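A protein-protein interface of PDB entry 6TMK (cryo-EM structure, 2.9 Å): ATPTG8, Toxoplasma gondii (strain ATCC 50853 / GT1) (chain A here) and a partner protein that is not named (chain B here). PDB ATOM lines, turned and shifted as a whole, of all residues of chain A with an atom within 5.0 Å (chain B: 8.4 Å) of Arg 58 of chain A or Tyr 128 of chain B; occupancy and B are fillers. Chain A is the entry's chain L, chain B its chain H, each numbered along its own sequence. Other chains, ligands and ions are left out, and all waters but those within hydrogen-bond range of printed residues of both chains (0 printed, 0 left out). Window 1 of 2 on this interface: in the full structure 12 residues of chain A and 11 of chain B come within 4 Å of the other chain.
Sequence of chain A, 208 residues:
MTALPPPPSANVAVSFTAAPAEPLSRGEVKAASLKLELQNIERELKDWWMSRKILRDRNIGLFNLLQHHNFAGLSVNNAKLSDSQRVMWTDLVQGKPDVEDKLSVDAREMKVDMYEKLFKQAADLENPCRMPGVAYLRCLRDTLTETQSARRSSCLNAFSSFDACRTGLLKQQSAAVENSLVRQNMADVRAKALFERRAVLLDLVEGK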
ATOM      1  N   LYS A  53      -6.530 -13.752  14.803  1.00  0.00           N
ATOM      2  CA  LYS A  53      -6.467 -12.353  14.399  1.00  0.00           C
ATOM      3  C   LYS A  53      -6.231 -11.440  15.595  1.00  0.00           C
ATOM      4  O   LYS A  53      -5.370 -10.550  15.556  1.00  0.00           O
ATOM      5  CB  LYS A  53      -7.764 -11.998  13.676  1.00  0.00           C
ATOM      6  CG  LYS A  53      -7.868 -10.605  13.145  1.00  0.00           C
ATOM      7  CD  LYS A  53      -7.073 -10.452  11.893  1.00  0.00           C
ATOM      8  CE  LYS A  53      -7.058  -9.023  11.429  1.00  0.00           C
ATOM      9  NZ  LYS A  53      -8.366  -8.649  10.886  1.00  0.00           N
ATOM     10  N   ILE A  54      -6.999 -11.636  16.669  1.00  0.00           N
ATOM     11  CA  ILE A  54      -6.883 -10.759  17.826  1.00  0.00           C
ATOM     12  C   ILE A  54      -5.499 -10.878  18.443  1.00  0.00           C
ATOM     13  O   ILE A  54      -4.881  -9.873  18.810  1.00  0.00           O
ATOM     14  CB  ILE A  54      -7.988 -11.062  18.852  1.00  0.00           C
ATOM     15  CG1 ILE A  54      -9.353 -10.725  18.280  1.00  0.00           C
ATOM     16  CG2 ILE A  54      -7.787 -10.252  20.101  1.00  0.00           C
ATOM     17  CD1 ILE A  54     -10.461 -11.454  18.928  1.00  0.00           C
ATOM     18  N   LEU A  55      -4.996 -12.105  18.580  1.00  0.00           N
ATOM     19  CA  LEU A  55      -3.685 -12.284  19.190  1.00  0.00           C
ATOM     20  C   LEU A  55      -2.583 -11.685  18.329  1.00  0.00           C
ATOM     21  O   LEU A  55      -1.666 -11.040  18.849  1.00  0.00           O
ATOM     22  CB  LEU A  55      -3.434 -13.763  19.446  1.00  0.00           C
ATOM     23  CG  LEU A  55      -4.079 -14.295  20.717  1.00  0.00           C
ATOM     24  CD1 LEU A  55      -4.077 -15.791  20.710  1.00  0.00           C
ATOM     25  CD2 LEU A  55      -3.365 -13.778  21.938  1.00  0.00           C
ATOM     26  N   ARG A  56      -2.653 -11.879  17.013  1.00  0.00           N
ATOM     27  CA  ARG A  56      -1.674 -11.272  16.122  1.00  0.00           C
ATOM     28  C   ARG A  56      -1.658  -9.761  16.280  1.00  0.00           C
ATOM     29  O   ARG A  56      -0.593  -9.149  16.434  1.00  0.00           O
ATOM     30  CB  ARG A  56      -1.977 -11.660  14.682  1.00  0.00           C
ATOM     31  CG  ARG A  56      -0.815 -11.511  13.740  1.00  0.00           C
ATOM     32  CD  ARG A  56      -1.232 -11.780  12.326  1.00  0.00           C
ATOM     33  NE  ARG A  56      -0.544 -10.923  11.372  1.00  0.00           N
ATOM     34  CZ  ARG A  56       0.741 -11.030  11.071  1.00  0.00           C
ATOM     35  NH1 ARG A  56       1.483 -11.958  11.649  1.00  0.00           N
ATOM     36  NH2 ARG A  56       1.280 -10.207  10.192  1.00  0.00           N
ATOM     37  N   ASP A  57      -2.835  -9.139  16.248  1.00  0.00           N
ATOM     38  CA  ASP A  57      -2.908  -7.687  16.351  1.00  0.00           C
ATOM     39  C   ASP A  57      -2.370  -7.205  17.692  1.00  0.00           C
ATOM     40  O   ASP A  57      -1.579  -6.257  17.753  1.00  0.00           O
ATOM     41  CB  ASP A  57      -4.343  -7.222  16.137  1.00  0.00           C
ATOM     42  CG  ASP A  57      -4.788  -7.351  14.692  1.00  0.00           C
ATOM     43  OD1 ASP A  57      -5.960  -7.038  14.399  1.00  0.00           O
ATOM     44  OD2 ASP A  57      -3.964  -7.760  13.847  1.00  0.00           O
ATOM     45  N   ARG A  58      -2.782  -7.852  18.782  1.00  0.00           N
ATOM     46  CA  ARG A  58      -2.330  -7.440  20.103  1.00  0.00           C
ATOM     47  C   ARG A  58      -0.818  -7.542  20.219  1.00  0.00           C
ATOM     48  O   ARG A  58      -0.162  -6.634  20.740  1.00  0.00           O
ATOM     49  CB  ARG A  58      -2.998  -8.292  21.177  1.00  0.00           C
ATOM     50  CG  ARG A  58      -2.429  -8.074  22.557  1.00  0.00           C
ATOM     51  CD  ARG A  58      -3.217  -8.771  23.619  1.00  0.00           C
ATOM     52  NE  ARG A  58      -2.571  -8.647  24.917  1.00  0.00           N
ATOM     53  CZ  ARG A  58      -2.659  -7.578  25.696  1.00  0.00           C
ATOM     54  NH1 ARG A  58      -3.368  -6.535  25.321  1.00  0.00           N
ATOM     55  NH2 ARG A  58      -2.031  -7.550  26.852  1.00  0.00           N
ATOM     56  N   ASN A  59      -0.243  -8.649  19.755  1.00  0.00           N
ATOM     57  CA  ASN A  59       1.178  -8.857  19.967  1.00  0.00           C
ATOM     58  C   ASN A  59       2.014  -7.974  19.053  1.00  0.00           C
ATOM     59  O   ASN A  59       3.094  -7.525  19.450  1.00  0.00           O
ATOM     60  CB  ASN A  59       1.510 -10.328  19.762  1.00  0.00           C
ATOM     61  CG  ASN A  59       0.857 -11.208  20.796  1.00  0.00           C
ATOM     62  OD1 ASN A  59       0.075 -12.095  20.474  1.00  0.00           O
ATOM     63  ND2 ASN A  59       1.153 -10.946  22.052  1.00  0.00           N
ATOM     64  N   ILE A  60       1.524  -7.672  17.852  1.00  0.00           N
ATOM     65  CA  ILE A  60       2.221  -6.702  17.017  1.00  0.00           C
ATOM     66  C   ILE A  60       2.159  -5.319  17.649  1.00  0.00           C
ATOM     67  O   ILE A  60       3.133  -4.558  17.602  1.00  0.00           O
ATOM     68  CB  ILE A  60       1.654  -6.711  15.590  1.00  0.00           C
ATOM     69  CG1 ILE A  60       2.208  -7.905  14.822  1.00  0.00           C
ATOM     70  CG2 ILE A  60       2.012  -5.445  14.871  1.00  0.00           C
ATOM     71  CD1 ILE A  60       1.369  -8.341  13.692  1.00  0.00           C
ATOM     72  N   GLY A  61       1.025  -4.971  18.255  1.00  0.00           N
ATOM     73  CA  GLY A  61       0.942  -3.700  18.948  1.00  0.00           C
ATOM     74  C   GLY A  61       1.898  -3.613  20.120  1.00  0.00           C
ATOM     75  O   GLY A  61       2.534  -2.580  20.337  1.00  0.00           O
ATOM     76  N   LEU A  62       2.005  -4.689  20.897  1.00  0.00           N
ATOM     77  CA  LEU A  62       2.982  -4.725  21.982  1.00  0.00           C
ATOM     78  C   LEU A  62       4.400  -4.570  21.457  1.00  0.00           C
ATOM     79  O   LEU A  62       5.210  -3.842  22.038  1.00  0.00           O
ATOM     80  CB  LEU A  62       2.861  -6.012  22.789  1.00  0.00           C
ATOM     81  CG  LEU A  62       1.663  -6.188  23.698  1.00  0.00           C
ATOM     82  CD1 LEU A  62       1.636  -7.575  24.248  1.00  0.00           C
ATOM     83  CD2 LEU A  62       1.802  -5.206  24.824  1.00  0.00           C
ATOM     84  N   PRO B  76     -19.410  -5.426  28.775  1.00  0.00           N
ATOM     85  CA  PRO B  76     -19.805  -5.935  27.457  1.00  0.00           C
ATOM     86  C   PRO B  76     -20.832  -7.046  27.532  1.00  0.00           C
ATOM     87  O   PRO B  76     -21.644  -7.193  26.610  1.00  0.00           O
ATOM     88  CB  PRO B  76     -18.480  -6.426  26.863  1.00  0.00           C
ATOM     89  CG  PRO B  76     -17.443  -5.728  27.606  1.00  0.00           C
ATOM     90  CD  PRO B  76     -17.961  -5.531  28.985  1.00  0.00           C
ATOM     91  N   TRP B  77     -20.817  -7.833  28.596  1.00  0.00           N
ATOM     92  CA  TRP B  77     -21.735  -8.943  28.764  1.00  0.00           C
ATOM     93  C   TRP B  77     -22.958  -8.509  29.561  1.00  0.00           C
ATOM     94  O   TRP B  77     -22.955  -7.488  30.248  1.00  0.00           O
ATOM     95  CB  TRP B  77     -21.033 -10.110  29.457  1.00  0.00           C
ATOM     96  CG  TRP B  77     -20.422  -9.772  30.770  1.00  0.00           C
ATOM     97  CD1 TRP B  77     -21.017  -9.833  31.987  1.00  0.00           C
ATOM     98  CD2 TRP B  77     -19.089  -9.312  30.999  1.00  0.00           C
ATOM     99  NE1 TRP B  77     -20.141  -9.443  32.964  1.00  0.00           N
ATOM    100  CE2 TRP B  77     -18.948  -9.118  32.380  1.00  0.00           C
ATOM    101  CE3 TRP B  77     -17.999  -9.050  30.170  1.00  0.00           C
ATOM    102  CZ2 TRP B  77     -17.766  -8.677  32.949  1.00  0.00           C
ATOM    103  CZ3 TRP B  77     -16.838  -8.613  30.736  1.00  0.00           C
ATOM    104  CH2 TRP B  77     -16.727  -8.427  32.111  1.00  0.00           C
ATOM    105  N   PHE B 118     -18.265 -16.829  29.131  1.00  0.00           N
ATOM    106  CA  PHE B 118     -18.055 -16.486  27.736  1.00  0.00           C
ATOM    107  C   PHE B 118     -18.404 -17.662  26.836  1.00  0.00           C
ATOM    108  O   PHE B 118     -18.020 -18.803  27.108  1.00  0.00           O
ATOM    109  CB  PHE B 118     -16.602 -16.081  27.514  1.00  0.00           C
ATOM    110  CG  PHE B 118     -16.269 -14.706  27.988  1.00  0.00           C
ATOM    111  CD1 PHE B 118     -16.783 -13.598  27.357  1.00  0.00           C
ATOM    112  CD2 PHE B 118     -15.430 -14.522  29.064  1.00  0.00           C
ATOM    113  CE1 PHE B 118     -16.467 -12.341  27.792  1.00  0.00           C
ATOM    114  CE2 PHE B 118     -15.115 -13.264  29.496  1.00  0.00           C
ATOM    115  CZ  PHE B 118     -15.634 -12.174  28.860  1.00  0.00           C
ATOM    116  N   ASN B 121     -13.679 -18.189  23.252  1.00  0.00           N
ATOM    117  CA  ASN B 121     -12.410 -17.730  23.797  1.00  0.00           C
ATOM    118  C   ASN B 121     -12.015 -16.362  23.255  1.00  0.00           C
ATOM    119  O   ASN B 121     -11.328 -15.598  23.944  1.00  0.00           O
ATOM    120  CB  ASN B 121     -11.323 -18.756  23.501  1.00  0.00           C
ATOM    121  CG  ASN B 121      -9.983 -18.368  24.082  1.00  0.00           C
ATOM    122  OD1 ASN B 121      -9.899 -17.840  25.190  1.00  0.00           O
ATOM    123  ND2 ASN B 121      -8.923 -18.621  23.330  1.00  0.00           N
ATOM    124  N   TRP B 122     -12.442 -16.028  22.039  1.00  0.00           N
ATOM    125  CA  TRP B 122     -12.036 -14.762  21.452  1.00  0.00           C
ATOM    126  C   TRP B 122     -12.763 -13.591  22.095  1.00  0.00           C
ATOM    127  O   TRP B 122     -12.224 -12.481  22.141  1.00  0.00           O
ATOM    128  CB  TRP B 122     -12.249 -14.779  19.939  1.00  0.00           C
ATOM    129  CG  TRP B 122     -13.653 -14.933  19.481  1.00  0.00           C
ATOM    130  CD1 TRP B 122     -14.293 -16.095  19.192  1.00  0.00           C
ATOM    131  CD2 TRP B 122     -14.589 -13.885  19.222  1.00  0.00           C
ATOM    132  NE1 TRP B 122     -15.573 -15.839  18.781  1.00  0.00           N
ATOM    133  CE2 TRP B 122     -15.779 -14.488  18.792  1.00  0.00           C
ATOM    134  CE3 TRP B 122     -14.538 -12.493  19.320  1.00  0.00           C
ATOM    135  CZ2 TRP B 122     -16.903 -13.755  18.464  1.00  0.00           C
ATOM    136  CZ3 TRP B 122     -15.655 -11.771  18.994  1.00  0.00           C
ATOM    137  CH2 TRP B 122     -16.822 -12.398  18.570  1.00  0.00           C
ATOM    138  N   GLU B 123     -13.963 -13.816  22.625  1.00  0.00           N
ATOM    139  CA  GLU B 123     -14.639 -12.780  23.395  1.00  0.00           C
ATOM    140  C   GLU B 123     -13.861 -12.461  24.663  1.00  0.00           C
ATOM    141  O   GLU B 123     -13.680 -11.294  25.026  1.00  0.00           O
ATOM    142  CB  GLU B 123     -16.052 -13.238  23.732  1.00  0.00           C
ATOM    143  CG  GLU B 123     -16.960 -13.330  22.541  1.00  0.00           C
ATOM    144  CD  GLU B 123     -18.194 -14.165  22.809  1.00  0.00           C
ATOM    145  OE1 GLU B 123     -18.542 -14.357  23.993  1.00  0.00           O
ATOM    146  OE2 GLU B 123     -18.814 -14.638  21.834  1.00  0.00           O
ATOM    147  N   ARG B 124     -13.417 -13.502  25.362  1.00  0.00           N
ATOM    148  CA  ARG B 124     -12.553 -13.338  26.521  1.00  0.00           C
ATOM    149  C   ARG B 124     -11.304 -12.551  26.156  1.00  0.00           C
ATOM    150  O   ARG B 124     -10.927 -11.587  26.839  1.00  0.00           O
ATOM    151  CB  ARG B 124     -12.192 -14.721  27.046  1.00  0.00           C
ATOM    152  CG  ARG B 124     -11.585 -14.785  28.412  1.00  0.00           C
ATOM    153  CD  ARG B 124     -11.164 -16.208  28.712  1.00  0.00           C
ATOM    154  NE  ARG B 124     -12.308 -17.075  28.960  1.00  0.00           N
ATOM    155  CZ  ARG B 124     -12.891 -17.228  30.141  1.00  0.00           C
ATOM    156  NH1 ARG B 124     -12.444 -16.573  31.200  1.00  0.00           N
ATOM    157  NH2 ARG B 124     -13.928 -18.039  30.262  1.00  0.00           N
ATOM    158  N   LEU B 125     -10.645 -12.961  25.074  1.00  0.00           N
ATOM    159  CA  LEU B 125      -9.453 -12.271  24.603  1.00  0.00           C
ATOM    160  C   LEU B 125      -9.722 -10.796  24.351  1.00  0.00           C
ATOM    161  O   LEU B 125      -8.944  -9.937  24.764  1.00  0.00           O
ATOM    162  CB  LEU B 125      -8.950 -12.940  23.333  1.00  0.00           C
ATOM    163  CG  LEU B 125      -7.955 -14.066  23.519  1.00  0.00           C
ATOM    164  CD1 LEU B 125      -7.911 -14.907  22.273  1.00  0.00           C
ATOM    165  CD2 LEU B 125      -6.606 -13.458  23.812  1.00  0.00           C
ATOM    166  N   LEU B 126     -10.806 -10.488  23.646  1.00  0.00           N
ATOM    167  CA  LEU B 126     -11.086  -9.110  23.277  1.00  0.00           C
ATOM    168  C   LEU B 126     -11.408  -8.260  24.497  1.00  0.00           C
ATOM    169  O   LEU B 126     -10.959  -7.111  24.600  1.00  0.00           O
ATOM    170  CB  LEU B 126     -12.230  -9.077  22.274  1.00  0.00           C
ATOM    171  CG  LEU B 126     -12.343  -7.821  21.422  1.00  0.00           C
ATOM    172  CD1 LEU B 126     -11.198  -7.695  20.463  1.00  0.00           C
ATOM    173  CD2 LEU B 126     -13.637  -7.860  20.692  1.00  0.00           C
ATOM    174  N   ALA B 127     -12.181  -8.806  25.433  1.00  0.00           N
ATOM    175  CA  ALA B 127     -12.480  -8.081  26.659  1.00  0.00           C
ATOM    176  C   ALA B 127     -11.207  -7.767  27.431  1.00  0.00           C
ATOM    177  O   ALA B 127     -11.000  -6.632  27.880  1.00  0.00           O
ATOM    178  CB  ALA B 127     -13.441  -8.894  27.513  1.00  0.00           C
ATOM    179  N   TYR B 128     -10.331  -8.761  27.585  1.00  0.00           N
ATOM    180  CA  TYR B 128      -9.061  -8.511  28.251  1.00  0.00           C
ATOM    181  C   TYR B 128      -8.238  -7.472  27.504  1.00  0.00           C
ATOM    182  O   TYR B 128      -7.670  -6.559  28.113  1.00  0.00           O
ATOM    183  CB  TYR B 128      -8.273  -9.810  28.376  1.00  0.00           C
ATOM    184  CG  TYR B 128      -6.884  -9.596  28.918  1.00  0.00           C
ATOM    185  CD1 TYR B 128      -6.677  -9.316  30.253  1.00  0.00           C
ATOM    186  CD2 TYR B 128      -5.783  -9.635  28.084  1.00  0.00           C
ATOM    187  CE1 TYR B 128      -5.420  -9.105  30.744  1.00  0.00           C
ATOM    188  CE2 TYR B 128      -4.524  -9.423  28.566  1.00  0.00           C
ATOM    189  CZ  TYR B 128      -4.344  -9.155  29.898  1.00  0.00           C
ATOM    190  OH  TYR B 128      -3.079  -8.941  30.386  1.00  0.00           O
ATOM    191  N   HIS B 129      -8.176  -7.594  26.182  1.00  0.00           N
ATOM    192  CA  HIS B 129      -7.374  -6.694  25.372  1.00  0.00           C
ATOM    193  C   HIS B 129      -7.844  -5.256  25.498  1.00  0.00           C
ATOM    194  O   HIS B 129      -7.032  -4.329  25.425  1.00  0.00           O
ATOM    195  CB  HIS B 129      -7.418  -7.160  23.921  1.00  0.00           C
ATOM    196  CG  HIS B 129      -6.824  -6.195  22.952  1.00  0.00           C
ATOM    197  ND1 HIS B 129      -5.465  -6.034  22.807  1.00  0.00           N
ATOM    198  CD2 HIS B 129      -7.400  -5.338  22.081  1.00  0.00           C
ATOM    199  CE1 HIS B 129      -5.230  -5.125  21.881  1.00  0.00           C
ATOM    200  NE2 HIS B 129      -6.388  -4.685  21.428  1.00  0.00           N
ATOM    201  N   HIS B 130      -9.138  -5.045  25.685  1.00  0.00           N
ATOM    202  CA  HIS B 130      -9.666  -3.700  25.829  1.00  0.00           C
ATOM    203  C   HIS B 130      -9.784  -3.252  27.275  1.00  0.00           C
ATOM    204  O   HIS B 130     -10.173  -2.107  27.522  1.00  0.00           O
ATOM    205  CB  HIS B 130     -11.020  -3.590  25.143  1.00  0.00           C
ATOM    206  CG  HIS B 130     -10.917  -3.353  23.674  1.00  0.00           C
ATOM    207  ND1 HIS B 130     -10.516  -2.149  23.144  1.00  0.00           N
ATOM    208  CD2 HIS B 130     -11.127  -4.176  22.626  1.00  0.00           C
ATOM    209  CE1 HIS B 130     -10.500  -2.237  21.829  1.00  0.00           C
ATOM    210  NE2 HIS B 130     -10.871  -3.455  21.489  1.00  0.00           N
ATOM    211  N   GLY B 131      -9.474  -4.117  28.229  1.00  0.00           N
ATOM    212  CA  GLY B 131      -9.423  -3.707  29.611  1.00  0.00           C
ATOM    213  C   GLY B 131     -10.734  -3.817  30.336  1.00  0.00           C
ATOM    214  O   GLY B 131     -11.021  -2.992  31.210  1.00  0.00           O
ATOM    215  N   LEU B 132     -11.541  -4.819  30.004  1.00  0.00           N
ATOM    216  CA  LEU B 132     -12.872  -4.966  30.561  1.00  0.00           C
ATOM    217  C   LEU B 132     -13.061  -6.305  31.249  1.00  0.00           C
ATOM    218  O   LEU B 132     -14.186  -6.639  31.630  1.00  0.00           O
ATOM    219  CB  LEU B 132     -13.905  -4.790  29.453  1.00  0.00           C
ATOM    220  CG  LEU B 132     -13.901  -3.430  28.766  1.00  0.00           C
ATOM    221  CD1 LEU B 132     -14.373  -3.554  27.348  1.00  0.00           C
ATOM    222  CD2 LEU B 132     -14.753  -2.455  29.509  1.00  0.00           C
ATOM    223  N   TYR B 133     -11.993  -7.075  31.430  1.00  0.00           N
ATOM    224  CA  TYR B 133     -12.094  -8.370  32.081  1.00  0.00           C
ATOM    225  C   TYR B 133     -10.738  -8.782  32.621  1.00  0.00           C
ATOM    226  O   TYR B 133      -9.730  -8.680  31.918  1.00  0.00           O
ATOM    227  CB  TYR B 133     -12.614  -9.434  31.119  1.00  0.00           C
ATOM    228  CG  TYR B 133     -12.444 -10.834  31.627  1.00  0.00           C
ATOM    229  CD1 TYR B 133     -13.257 -11.328  32.625  1.00  0.00           C
ATOM    230  CD2 TYR B 133     -11.469 -11.660  31.111  1.00  0.00           C
ATOM    231  CE1 TYR B 133     -13.103 -12.602  33.092  1.00  0.00           C
ATOM    232  CE2 TYR B 133     -11.309 -12.934  31.572  1.00  0.00           C
ATOM    233  CZ  TYR B 133     -12.129 -13.404  32.564  1.00  0.00           C
ATOM    234  OH  TYR B 133     -11.976 -14.683  33.034  1.00  0.00           O
ATOM    235  N   SER B 134     -10.721  -9.225  33.877  1.00  0.00           N
ATOM    236  CA  SER B 134      -9.601  -9.930  34.436  1.00  0.00           C
ATOM    237  C   SER B 134     -10.205 -10.977  35.367  1.00  0.00           C
ATOM    238  O   SER B 134     -11.061 -10.638  36.205  1.00  0.00           O
ATOM    239  CB  SER B 134      -8.642  -9.012  35.190  1.00  0.00           C
ATOM    240  OG  SER B 134      -9.030  -8.845  36.537  1.00  0.00           O
ATOM    241  N   PRO B 135      -9.812 -12.245  35.244  1.00  0.00           N
ATOM    242  CA  PRO B 135     -10.378 -13.260  36.141  1.00  0.00           C
ATOM    243  C   PRO B 135     -10.020 -13.029  37.591  1.00  0.00           C
ATOM    244  O   PRO B 135     -10.839 -13.301  38.479  1.00  0.00           O
ATOM    245  CB  PRO B 135      -9.792 -14.567  35.596  1.00  0.00           C
ATOM    246  CG  PRO B 135      -8.567 -14.171  34.895  1.00  0.00           C
ATOM    247  CD  PRO B 135      -8.800 -12.814  34.341  1.00  0.00           C
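NH1 of Arg 58 of chain A is in hydrogen-bond range of ND1 of His 129 of chain B, at 3.3 Å.
The backbone carbonyl oxygen (O) of Leu 55 of chain A lies close to the side-chain amide oxygen (OD1) of Asn 59 of chain A (2.6 Å).
Among the printed residues, merely in contact across the chains: Arg 58 of chain A with Tyr 128 of chain B (3.6 Å), Leu 55 of chain A with Leu 125 of chain B (3.8 Å) and Ile 54 of chain A with Trp 122 of chain B (3.8 Å).
Of the printed residues of chain B, Leu 55 of chain A touches Leu 125. Ile 60 of chain A touches none of the printed residues of chain B. Of the printed residues of chain A, Trp 122 of chain B touches Ile 54 (3.8 Å). Of the printed residues of chain A, Leu 125 of chain B touches Leu 55. Ala 127 of chain B touches none of the printed residues of chain A. Tyr 128 of chain B touches one residue of chain A. The nearest residue of chain B that does not touch Arg 58 of chain A is Leu 125 of chain B (5.8 Å). The nearest printed residue of chain A that does not touch His 129 of chain B is Ile 54 of chain A (4.9 Å).
Of the 18 printed residues of chain B, 4 touch a printed residue of chain A.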
